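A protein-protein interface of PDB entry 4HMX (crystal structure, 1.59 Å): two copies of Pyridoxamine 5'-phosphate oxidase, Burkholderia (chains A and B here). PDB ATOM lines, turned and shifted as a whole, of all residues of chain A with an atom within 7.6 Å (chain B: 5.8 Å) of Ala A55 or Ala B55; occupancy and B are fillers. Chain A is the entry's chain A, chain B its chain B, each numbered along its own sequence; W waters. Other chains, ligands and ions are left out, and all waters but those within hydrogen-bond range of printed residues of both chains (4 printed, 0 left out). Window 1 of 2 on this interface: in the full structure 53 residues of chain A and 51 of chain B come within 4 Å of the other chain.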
ATOM      1  N   LEU A  52      23.665  24.832  -2.974  1.00  0.00           N
ATOM      2  CA  LEU A  52      23.716  24.626  -1.530  1.00  0.00           C
ATOM      3  C   LEU A  52      22.623  23.682  -1.102  1.00  0.00           C
ATOM      4  O   LEU A  52      21.476  23.869  -1.502  1.00  0.00           O
ATOM      5  CB  LEU A  52      23.475  26.049  -0.903  1.00  0.00           C
ATOM      6  CG  LEU A  52      23.642  26.370   0.522  1.00  0.00           C
ATOM      7  CD1 LEU A  52      25.105  26.414   0.874  1.00  0.00           C
ATOM      8  CD2 LEU A  52      22.941  27.723   0.823  1.00  0.00           C
ATOM      9  N   ALA A  53      22.955  22.637  -0.347  1.00  0.00           N
ATOM     10  CA  ALA A  53      21.905  21.790   0.217  1.00  0.00           C
ATOM     11  C   ALA A  53      21.461  22.516   1.465  1.00  0.00           C
ATOM     12  O   ALA A  53      22.200  22.556   2.447  1.00  0.00           O
ATOM     13  CB  ALA A  53      22.461  20.430   0.579  1.00  0.00           C
ATOM     14  N   LEU A  54      20.282  23.100   1.412  1.00  0.00           N
ATOM     15  CA  LEU A  54      19.758  23.926   2.496  1.00  0.00           C
ATOM     16  C   LEU A  54      18.721  23.140   3.301  1.00  0.00           C
ATOM     17  O   LEU A  54      17.663  22.784   2.817  1.00  0.00           O
ATOM     18  CB  LEU A  54      19.057  25.183   1.949  1.00  0.00           C
ATOM     19  CG  LEU A  54      18.659  26.149   3.074  1.00  0.00           C
ATOM     20  CD1 LEU A  54      19.883  26.885   3.678  1.00  0.00           C
ATOM     21  CD2 LEU A  54      17.620  27.149   2.564  1.00  0.00           C
ATOM     22  N   ALA A  55      19.074  22.924   4.559  1.00  0.00           N
ATOM     23  CA  ALA A  55      18.185  22.267   5.494  1.00  0.00           C
ATOM     24  C   ALA A  55      17.523  23.283   6.395  1.00  0.00           C
ATOM     25  O   ALA A  55      18.174  24.207   6.870  1.00  0.00           O
ATOM     26  CB  ALA A  55      18.965  21.218   6.311  1.00  0.00           C
ATOM     27  N   THR A  56      16.248  23.010   6.684  1.00  0.00           N
ATOM     28  CA  THR A  56      15.435  23.819   7.587  1.00  0.00           C
ATOM     29  C   THR A  56      14.616  22.863   8.462  1.00  0.00           C
ATOM     30  O   THR A  56      14.571  21.657   8.212  1.00  0.00           O
ATOM     31  CB  THR A  56      14.467  24.783   6.798  1.00  0.00           C
ATOM     32  OG1 THR A  56      13.651  24.041   5.885  1.00  0.00           O
ATOM     33  CG2 THR A  56      15.257  25.800   5.951  1.00  0.00           C
ATOM     34  N   ALA A  57      13.914  23.390   9.446  1.00  0.00           N
ATOM     35  CA  ALA A  57      13.062  22.524  10.259  1.00  0.00           C
ATOM     36  C   ALA A  57      11.813  23.219  10.724  1.00  0.00           C
ATOM     37  O   ALA A  57      11.799  24.421  10.927  1.00  0.00           O
ATOM     38  CB  ALA A  57      13.804  21.980  11.478  1.00  0.00           C
ATOM     39  N   ILE A  63      13.084  17.771  10.006  1.00  0.00           N
ATOM     40  CA  ILE A  63      13.989  18.502   9.115  1.00  0.00           C
ATOM     41  C   ILE A  63      13.670  18.204   7.664  1.00  0.00           C
ATOM     42  O   ILE A  63      13.304  17.080   7.317  1.00  0.00           O
ATOM     43  CB  ILE A  63      15.474  18.073   9.397  1.00  0.00           C
ATOM     44  CG1 ILE A  63      15.778  18.246  10.896  1.00  0.00           C
ATOM     45  CG2 ILE A  63      16.476  18.855   8.588  1.00  0.00           C
ATOM     46  CD1 ILE A  63      17.163  17.792  11.275  1.00  0.00           C
ATOM     47  N   SER A  64      13.781  19.245   6.836  1.00  0.00           N
ATOM     48  CA  SER A  64      13.628  19.086   5.394  1.00  0.00           C
ATOM     49  C   SER A  64      14.822  19.764   4.683  1.00  0.00           C
ATOM     50  O   SER A  64      15.604  20.480   5.270  1.00  0.00           O
ATOM     51  CB  SER A  64      12.343  19.770   4.949  1.00  0.00           C
ATOM     52  OG  SER A  64      12.429  21.161   5.224  1.00  0.00           O
ATOM     53  N   SER A  65      14.999  19.406   3.427  1.00  0.00           N
ATOM     54  CA  SER A  65      16.135  19.851   2.679  1.00  0.00           C
ATOM     55  C   SER A  65      15.803  19.995   1.185  1.00  0.00           C
ATOM     56  O   SER A  65      14.908  19.349   0.650  1.00  0.00           O
ATOM     57  CB  SER A  65      17.327  18.905   2.907  1.00  0.00           C
ATOM     58  OG  SER A  65      18.507  19.501   2.398  1.00  0.00           O
ATOM     59  N   ARG A  66      16.514  20.895   0.550  1.00  0.00           N
ATOM     60  CA  ARG A  66      16.405  21.130  -0.922  1.00  0.00           C
ATOM     61  C   ARG A  66      17.617  21.916  -1.398  1.00  0.00           C
ATOM     62  O   ARG A  66      18.311  22.613  -0.602  1.00  0.00           O
ATOM     63  CB  ARG A  66      15.111  21.901  -1.311  1.00  0.00           C
ATOM     64  CG  ARG A  66      15.131  23.384  -0.980  1.00  0.00           C
ATOM     65  CD  ARG A  66      15.233  23.657   0.562  1.00  0.00           C
ATOM     66  NE  ARG A  66      13.987  23.232   1.173  1.00  0.00           N
ATOM     67  CZ  ARG A  66      13.810  23.099   2.481  1.00  0.00           C
ATOM     68  NH1 ARG A  66      12.612  22.758   2.939  1.00  0.00           N
ATOM     69  NH2 ARG A  66      14.825  23.244   3.353  1.00  0.00           N
ATOM     70  N   VAL A  67      17.910  21.827  -2.691  1.00  0.00           N
ATOM     71  CA  VAL A  67      18.974  22.637  -3.268  1.00  0.00           C
ATOM     72  C   VAL A  67      18.526  24.083  -3.447  1.00  0.00           C
ATOM     73  O   VAL A  67      17.412  24.349  -3.911  1.00  0.00           O
ATOM     74  CB  VAL A  67      19.422  22.073  -4.626  1.00  0.00           C
ATOM     75  CG1 VAL A  67      20.562  22.925  -5.257  1.00  0.00           C
ATOM     76  CG2 VAL A  67      19.899  20.623  -4.442  1.00  0.00           C
ATOM     77  N   ILE A  68      19.440  24.980  -3.132  1.00  0.00           N
ATOM     78  CA  ILE A  68      19.256  26.415  -3.357  1.00  0.00           C
ATOM     79  C   ILE A  68      20.541  26.927  -3.989  1.00  0.00           C
ATOM     80  O   ILE A  68      21.627  26.683  -3.454  1.00  0.00           O
ATOM     81  CB  ILE A  68      19.099  27.157  -1.992  1.00  0.00           C
ATOM     82  CG1 ILE A  68      17.807  26.677  -1.353  1.00  0.00           C
ATOM     83  CG2 ILE A  68      19.119  28.659  -2.197  1.00  0.00           C
ATOM     84  CD1 ILE A  68      16.587  27.176  -2.045  1.00  0.00           C
ATOM     85  N   LYS A  88       9.870  25.553   2.797  1.00  0.00           N
ATOM     86  CA  LYS A  88      11.044  26.086   3.484  1.00  0.00           C
ATOM     87  C   LYS A  88      10.716  27.480   4.079  1.00  0.00           C
ATOM     88  O   LYS A  88      11.163  27.866   5.163  1.00  0.00           O
ATOM     89  CB  LYS A  88      12.278  26.168   2.584  1.00  0.00           C
ATOM     90  CG  LYS A  88      12.436  27.484   1.787  1.00  0.00           C
ATOM     91  CD  LYS A  88      13.489  27.337   0.708  1.00  0.00           C
ATOM     92  CE  LYS A  88      13.086  26.436  -0.457  1.00  0.00           C
ATOM     93  NZ  LYS A  88      11.763  26.823  -0.973  1.00  0.00           N
ATOM     94  N   GLU A  91       8.953  27.161   7.291  1.00  0.00           N
ATOM     95  CA  GLU A  91       9.894  26.673   8.332  1.00  0.00           C
ATOM     96  C   GLU A  91      10.865  27.757   8.787  1.00  0.00           C
ATOM     97  O   GLU A  91      11.161  27.882   9.987  1.00  0.00           O
ATOM     98  CB  GLU A  91      10.636  25.437   7.809  1.00  0.00           C
ATOM     99  CG  GLU A  91       9.691  24.221   7.737  1.00  0.00           C
ATOM    100  CD  GLU A  91      10.293  22.913   7.291  1.00  0.00           C
ATOM    101  OE1 GLU A  91      11.531  22.827   7.112  1.00  0.00           O
ATOM    102  OE2 GLU A  91       9.481  21.941   7.223  1.00  0.00           O
ATOM    103  N   LEU A  92      11.330  28.564   7.833  1.00  0.00           N
ATOM    104  CA  LEU A  92      12.213  29.668   8.174  1.00  0.00           C
ATOM    105  C   LEU A  92      11.486  30.658   9.089  1.00  0.00           C
ATOM    106  O   LEU A  92      12.084  31.199  10.066  1.00  0.00           O
ATOM    107  CB  LEU A  92      12.752  30.351   6.904  1.00  0.00           C
ATOM    108  CG  LEU A  92      13.777  29.481   6.121  1.00  0.00           C
ATOM    109  CD1 LEU A  92      14.104  30.147   4.790  1.00  0.00           C
ATOM    110  CD2 LEU A  92      15.051  29.192   6.933  1.00  0.00           C
ATOM    111  N   GLY A  96      13.563  29.812  12.091  1.00  0.00           N
ATOM    112  CA  GLY A  96      14.731  30.598  11.736  1.00  0.00           C
ATOM    113  C   GLY A  96      16.009  29.838  11.394  1.00  0.00           C
ATOM    114  O   GLY A  96      16.836  30.324  10.675  1.00  0.00           O
ATOM    115  N   TRP A  97      16.170  28.650  11.918  1.00  0.00           N
ATOM    116  CA  TRP A  97      17.417  27.913  11.809  1.00  0.00           C
ATOM    117  C   TRP A  97      17.604  27.381  10.378  1.00  0.00           C
ATOM    118  O   TRP A  97      16.679  26.940   9.720  1.00  0.00           O
ATOM    119  CB  TRP A  97      17.444  26.765  12.833  1.00  0.00           C
ATOM    120  CG  TRP A  97      17.558  27.246  14.336  1.00  0.00           C
ATOM    121  CD1 TRP A  97      16.702  26.972  15.417  1.00  0.00           C
ATOM    122  CD2 TRP A  97      18.598  28.090  14.856  1.00  0.00           C
ATOM    123  NE1 TRP A  97      17.183  27.618  16.579  1.00  0.00           N
ATOM    124  CE2 TRP A  97      18.337  28.306  16.246  1.00  0.00           C
ATOM    125  CE3 TRP A  97      19.732  28.694  14.269  1.00  0.00           C
ATOM    126  CZ2 TRP A  97      19.183  29.092  17.046  1.00  0.00           C
ATOM    127  CZ3 TRP A  97      20.565  29.470  15.047  1.00  0.00           C
ATOM    128  CH2 TRP A  97      20.286  29.669  16.424  1.00  0.00           C
ATOM    129  N   ALA A  98      18.824  27.431   9.889  1.00  0.00           N
ATOM    130  CA  ALA A  98      19.126  26.787   8.597  1.00  0.00           C
ATOM    131  C   ALA A  98      20.556  26.298   8.568  1.00  0.00           C
ATOM    132  O   ALA A  98      21.399  26.800   9.290  1.00  0.00           O
ATOM    133  CB  ALA A  98      18.884  27.705   7.448  1.00  0.00           C
ATOM    134  N   SER A  99      20.819  25.295   7.726  1.00  0.00           N
ATOM    135  CA  SER A  99      22.188  24.852   7.485  1.00  0.00           C
ATOM    136  C   SER A  99      22.322  24.588   6.030  1.00  0.00           C
ATOM    137  O   SER A  99      21.537  23.852   5.451  1.00  0.00           O
ATOM    138  CB  SER A  99      22.486  23.563   8.263  1.00  0.00           C
ATOM    139  OG  SER A  99      23.806  23.130   8.141  1.00  0.00           O
ATOM    140  N   GLY A 100      23.328  25.223   5.464  1.00  0.00           N
ATOM    141  CA  GLY A 100      23.604  25.028   4.051  1.00  0.00           C
ATOM    142  C   GLY A 100      24.927  24.360   3.837  1.00  0.00           C
ATOM    143  O   GLY A 100      25.907  24.643   4.536  1.00  0.00           O
ATOM    144  N   LEU A 101      24.951  23.401   2.907  1.00  0.00           N
ATOM    145  CA  LEU A 101      26.135  22.602   2.655  1.00  0.00           C
ATOM    146  C   LEU A 101      26.534  22.668   1.187  1.00  0.00           C
ATOM    147  O   LEU A 101      25.715  22.365   0.305  1.00  0.00           O
ATOM    148  CB  LEU A 101      25.890  21.140   3.051  1.00  0.00           C
ATOM    149  CG  LEU A 101      27.082  20.194   2.954  1.00  0.00           C
ATOM    150  CD1 LEU A 101      28.178  20.505   4.024  1.00  0.00           C
ATOM    151  CD2 LEU A 101      26.593  18.729   3.059  1.00  0.00           C
ATOM    152  N   ILE A 113      27.611  25.908   6.342  1.00  0.00           N
ATOM    153  CA  ILE A 113      27.250  27.233   6.856  1.00  0.00           C
ATOM    154  C   ILE A 113      25.964  27.072   7.654  1.00  0.00           C
ATOM    155  O   ILE A 113      24.886  26.851   7.056  1.00  0.00           O
ATOM    156  CB  ILE A 113      27.029  28.258   5.690  1.00  0.00           C
ATOM    157  CG1 ILE A 113      28.231  28.177   4.763  1.00  0.00           C
ATOM    158  CG2 ILE A 113      26.843  29.629   6.328  1.00  0.00           C
ATOM    159  CD1 ILE A 113      28.036  28.466   3.298  1.00  0.00           C
ATOM    160  N   GLY A 115      23.318  28.691  10.688  1.00  0.00           N
ATOM    161  CA  GLY A 115      22.990  29.894  11.455  1.00  0.00           C
ATOM    162  C   GLY A 115      21.534  30.217  11.292  1.00  0.00           C
ATOM    163  O   GLY A 115      20.731  29.300  11.103  1.00  0.00           O
ATOM    164  N   LEU A 180      21.543  34.187   5.281  1.00  0.00           N
ATOM    165  CA  LEU A 180      21.959  33.160   6.232  1.00  0.00           C
ATOM    166  C   LEU A 180      23.186  33.681   6.967  1.00  0.00           C
ATOM    167  O   LEU A 180      24.245  33.755   6.380  1.00  0.00           O
ATOM    168  CB  LEU A 180      22.228  31.851   5.488  1.00  0.00           C
ATOM    169  CG  LEU A 180      22.702  30.685   6.287  1.00  0.00           C
ATOM    170  CD1 LEU A 180      21.793  30.500   7.454  1.00  0.00           C
ATOM    171  CD2 LEU A 180      22.899  29.437   5.468  1.00  0.00           C
ATOM    172  N   ALA B  53      23.680  14.846   1.459  1.00  0.00           N
ATOM    173  CA  ALA B  53      23.832  15.941   2.417  1.00  0.00           C
ATOM    174  C   ALA B  53      22.900  15.629   3.578  1.00  0.00           C
ATOM    175  O   ALA B  53      21.683  15.735   3.448  1.00  0.00           O
ATOM    176  CB  ALA B  53      23.458  17.302   1.767  1.00  0.00           C
ATOM    177  N   LEU B  54      23.480  15.169   4.690  1.00  0.00           N
ATOM    178  CA  LEU B  54      22.693  14.719   5.823  1.00  0.00           C
ATOM    179  C   LEU B  54      22.663  15.849   6.868  1.00  0.00           C
ATOM    180  O   LEU B  54      23.708  16.251   7.403  1.00  0.00           O
ATOM    181  CB  LEU B  54      23.358  13.509   6.486  1.00  0.00           C
ATOM    182  CG  LEU B  54      22.557  12.900   7.653  1.00  0.00           C
ATOM    183  CD1 LEU B  54      21.303  12.196   7.160  1.00  0.00           C
ATOM    184  CD2 LEU B  54      23.435  11.972   8.423  1.00  0.00           C
ATOM    185  N   ALA B  55      21.457  16.249   7.188  1.00  0.00           N
ATOM    186  CA  ALA B  55      21.146  17.261   8.217  1.00  0.00           C
ATOM    187  C   ALA B  55      20.521  16.630   9.473  1.00  0.00           C
ATOM    188  O   ALA B  55      19.632  15.775   9.399  1.00  0.00           O
ATOM    189  CB  ALA B  55      20.234  18.327   7.664  1.00  0.00           C
ATOM    190  N   THR B  56      21.021  17.141  10.593  1.00  0.00           N
ATOM    191  CA  THR B  56      20.611  16.709  11.901  1.00  0.00           C
ATOM    192  C   THR B  56      20.474  17.960  12.759  1.00  0.00           C
ATOM    193  O   THR B  56      20.927  19.031  12.358  1.00  0.00           O
ATOM    194  CB  THR B  56      21.679  15.724  12.545  1.00  0.00           C
ATOM    195  OG1 THR B  56      22.965  16.351  12.607  1.00  0.00           O
ATOM    196  CG2 THR B  56      21.784  14.434  11.759  1.00  0.00           C
ATOM    197  N   ALA B  57      19.893  17.834  13.948  1.00  0.00           N
ATOM    198  CA  ALA B  57      19.784  19.038  14.803  1.00  0.00           C
ATOM    199  C   ALA B  57      19.983  18.731  16.271  1.00  0.00           C
ATOM    200  O   ALA B  57      19.732  17.611  16.741  1.00  0.00           O
ATOM    201  CB  ALA B  57      18.471  19.671  14.630  1.00  0.00           C
ATOM    202  N   ILE B  63      20.635  23.378  13.388  1.00  0.00           N
ATOM    203  CA  ILE B  63      20.815  22.334  12.375  1.00  0.00           C
ATOM    204  C   ILE B  63      22.280  22.330  11.928  1.00  0.00           C
ATOM    205  O   ILE B  63      22.927  23.410  11.859  1.00  0.00           O
ATOM    206  CB  ILE B  63      19.897  22.603  11.172  1.00  0.00           C
ATOM    207  CG1 ILE B  63      18.430  22.728  11.609  1.00  0.00           C
ATOM    208  CG2 ILE B  63      20.061  21.529  10.113  1.00  0.00           C
ATOM    209  CD1 ILE B  63      17.500  23.106  10.481  1.00  0.00           C
ATOM    210  N   SER B  64      22.827  21.119  11.727  1.00  0.00           N
ATOM    211  CA  SER B  64      24.156  20.968  11.156  1.00  0.00           C
ATOM    212  C   SER B  64      24.039  19.996   9.972  1.00  0.00           C
ATOM    213  O   SER B  64      23.031  19.263   9.843  1.00  0.00           O
ATOM    214  CB  SER B  64      25.163  20.400  12.172  1.00  0.00           C
ATOM    215  OG  SER B  64      24.715  19.138  12.635  1.00  0.00           O
ATOM    216  N   SER B  65      25.012  20.029   9.082  1.00  0.00           N
ATOM    217  CA  SER B  65      24.937  19.180   7.908  1.00  0.00           C
ATOM    218  C   SER B  65      26.352  18.793   7.444  1.00  0.00           C
ATOM    219  O   SER B  65      27.326  19.458   7.770  1.00  0.00           O
ATOM    220  CB  SER B  65      24.069  19.794   6.821  1.00  0.00           C
ATOM    221  OG  SER B  65      24.580  21.009   6.400  1.00  0.00           O
ATOM    222  N   ARG B  66      26.439  17.683   6.712  1.00  0.00           N
ATOM    223  CA  ARG B  66      27.689  17.186   6.168  1.00  0.00           C
ATOM    224  C   ARG B  66      27.356  16.121   5.134  1.00  0.00           C
ATOM    225  O   ARG B  66      26.249  15.546   5.147  1.00  0.00           O
ATOM    226  CB  ARG B  66      28.555  16.542   7.242  1.00  0.00           C
ATOM    227  CG  ARG B  66      28.081  15.159   7.820  1.00  0.00           C
ATOM    228  CD  ARG B  66      26.788  15.234   8.530  1.00  0.00           C
ATOM    229  NE  ARG B  66      26.887  16.019   9.750  1.00  0.00           N
ATOM    230  CZ  ARG B  66      25.888  16.413  10.523  1.00  0.00           C
ATOM    231  NH1 ARG B  66      24.614  16.278  10.152  1.00  0.00           N
ATOM    232  NH2 ARG B  66      26.188  16.992  11.691  1.00  0.00           N
ATOM    233  N   TRP B  97      15.308  13.013  14.504  1.00  0.00           N
ATOM    234  CA  TRP B  97      14.968  13.411  13.141  1.00  0.00           C
ATOM    235  C   TRP B  97      16.218  13.711  12.285  1.00  0.00           C
ATOM    236  O   TRP B  97      17.214  14.252  12.781  1.00  0.00           O
ATOM    237  CB  TRP B  97      14.090  14.669  13.115  1.00  0.00           C
ATOM    238  CG  TRP B  97      12.825  14.621  13.917  1.00  0.00           C
ATOM    239  CD1 TRP B  97      12.583  15.328  15.053  1.00  0.00           C
ATOM    240  CD2 TRP B  97      11.616  13.916  13.607  1.00  0.00           C
ATOM    241  NE1 TRP B  97      11.321  15.071  15.495  1.00  0.00           N
ATOM    242  CE2 TRP B  97      10.704  14.194  14.646  1.00  0.00           C
ATOM    243  CE3 TRP B  97      11.222  13.066  12.573  1.00  0.00           C
ATOM    244  CZ2 TRP B  97       9.415  13.717  14.645  1.00  0.00           C
ATOM    245  CZ3 TRP B  97       9.931  12.517  12.632  1.00  0.00           C
ATOM    246  CH2 TRP B  97       9.059  12.852  13.647  1.00  0.00           C
ATOM    247  N   ALA B  98      16.159  13.362  10.998  1.00  0.00           N
ATOM    248  CA  ALA B  98      17.239  13.683  10.068  1.00  0.00           C
ATOM    249  C   ALA B  98      16.647  13.862   8.675  1.00  0.00           C
ATOM    250  O   ALA B  98      15.545  13.407   8.379  1.00  0.00           O
ATOM    251  CB  ALA B  98      18.270  12.586  10.012  1.00  0.00           C
ATOM    252  N   SER B  99      17.390  14.563   7.840  1.00  0.00           N
ATOM    253  CA  SER B  99      17.008  14.676   6.454  1.00  0.00           C
ATOM    254  C   SER B  99      18.230  14.529   5.604  1.00  0.00           C
ATOM    255  O   SER B  99      19.275  15.095   5.907  1.00  0.00           O
ATOM    256  CB  SER B  99      16.374  16.043   6.204  1.00  0.00           C
ATOM    257  OG  SER B  99      15.947  16.153   4.840  1.00  0.00           O
ATOM    258  N   GLY B 100      18.096  13.790   4.516  1.00  0.00           N
ATOM    259  CA  GLY B 100      19.189  13.627   3.571  1.00  0.00           C
ATOM    260  C   GLY B 100      18.793  14.091   2.198  1.00  0.00           C
ATOM    261  O   GLY B 100      17.683  13.843   1.803  1.00  0.00           O
HETATM  262  O   HOH W   1      21.399  25.980  12.241  1.00  0.00           O
HETATM  263  O   HOH W   2      13.015  14.794   9.533  1.00  0.00           O
HETATM  264  O   HOH W   3      22.194  20.437   4.354  1.00  0.00           O
HETATM  265  O   HOH W   4      20.484  18.369   3.819  1.00  0.00           O
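Ala A55 touches two residues of chain B.
Of the printed residues of chain B, Ser A65 touches Ser B99 (3.6 Å).
Printed residues of chain B within 4 Å of Ser A99: Ile B63 (3.6 Å), Ser B64 (3.6 Å) and Ser B65 (2.9 Å).
Of the printed residues of chain A, Arg B66 touches Leu A101 (3.4 Å).
Water W4 lies within hydrogen-bond range of OG of Ser A65 and O of Ala B53.
Water W3 bridges O of Ala A53 and OG of Ser B65.
Water W1 bridges the backbone NH (N) of Ile B63 and the backbone carbonyl oxygen (O) of Ala A98.
Water W2 bridges N of Ile A63 (3.0 Å) and O of Ala B98 (3.1 Å).
The backbone NH of Ala A53 lies within hydrogen-bond range of the backbone carbonyl oxygen of Leu A101.
The side-chain hydroxyl (OG) of Ser B64 sits at hydrogen-bond distance from the guanidinium group (NH2) of Arg B66.
The guanidinium group (NH2) of Arg A66 lies within hydrogen-bond range of the side-chain hydroxyl (OG1) of Thr A56, 2.9 Å away.
N of Ser B64 sits at hydrogen-bond distance from O of Thr B56 (2.9 Å).
NH1 of Arg B66 sits at hydrogen-bond distance from OG1 of Thr B56 (3.0 Å).
O of Thr A56 lies within hydrogen-bond range of N of Ser A64, at 2.9 Å.
The side-chain hydroxyl of Ser B65 lies within hydrogen-bond range of the side-chain hydroxyl of Ser A99 (2.9 Å).
Of the 13 printed residues of chain B, 10 touch a printed residue of chain A.
Along chain A the printed residues that touch a printed residue of chain B span positions 53 to 101.
Thr A56 touches Ile B63, and with the chains exchanged Ile A63 touches Thr B56.
Ala A57 touches Ile B63, and with the chains exchanged Ile A63 touches Ala B57.
Ile A63 touches Ser B99, and with the chains exchanged Ser A99 touches Ile B63.
Ser A64 touches Ser B99, and with the chains exchanged Ser A99 touches Ser B64.
Positions printed for both chains: 53, 54, 55, 56, 57, 63, 64, 65, 66, 97, 98, 99 and 100.
Of the 19 pairs that touch across the chains among the printed residues, 16 have their exchanged pair printed and touching as well.
Ala A55 touches Ala B55 (CB to CB, 3.4 Å).
O of Ala A55 touches CD1 of Ile B63, 3.8 Å away.
C of Thr A56 touches CD1 of Ile B63, at 3.5 Å.
CD1 of Ile B63 touches N of Ala A57 (3.7 Å).
Trp B97 touches Ile A63.
Ser A64 touches Ser B99 (CA to OG, 3.8 Å).
Ser A65 touches Ser B99 (CB to OG, 3.6 Å).
CD1 of Ile B63 touches O of Trp A97, 3.99 Å away.
Ser A99 touches Ile B63 (CB to O, 3.6 Å).
Arg B66 touches Leu A101.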
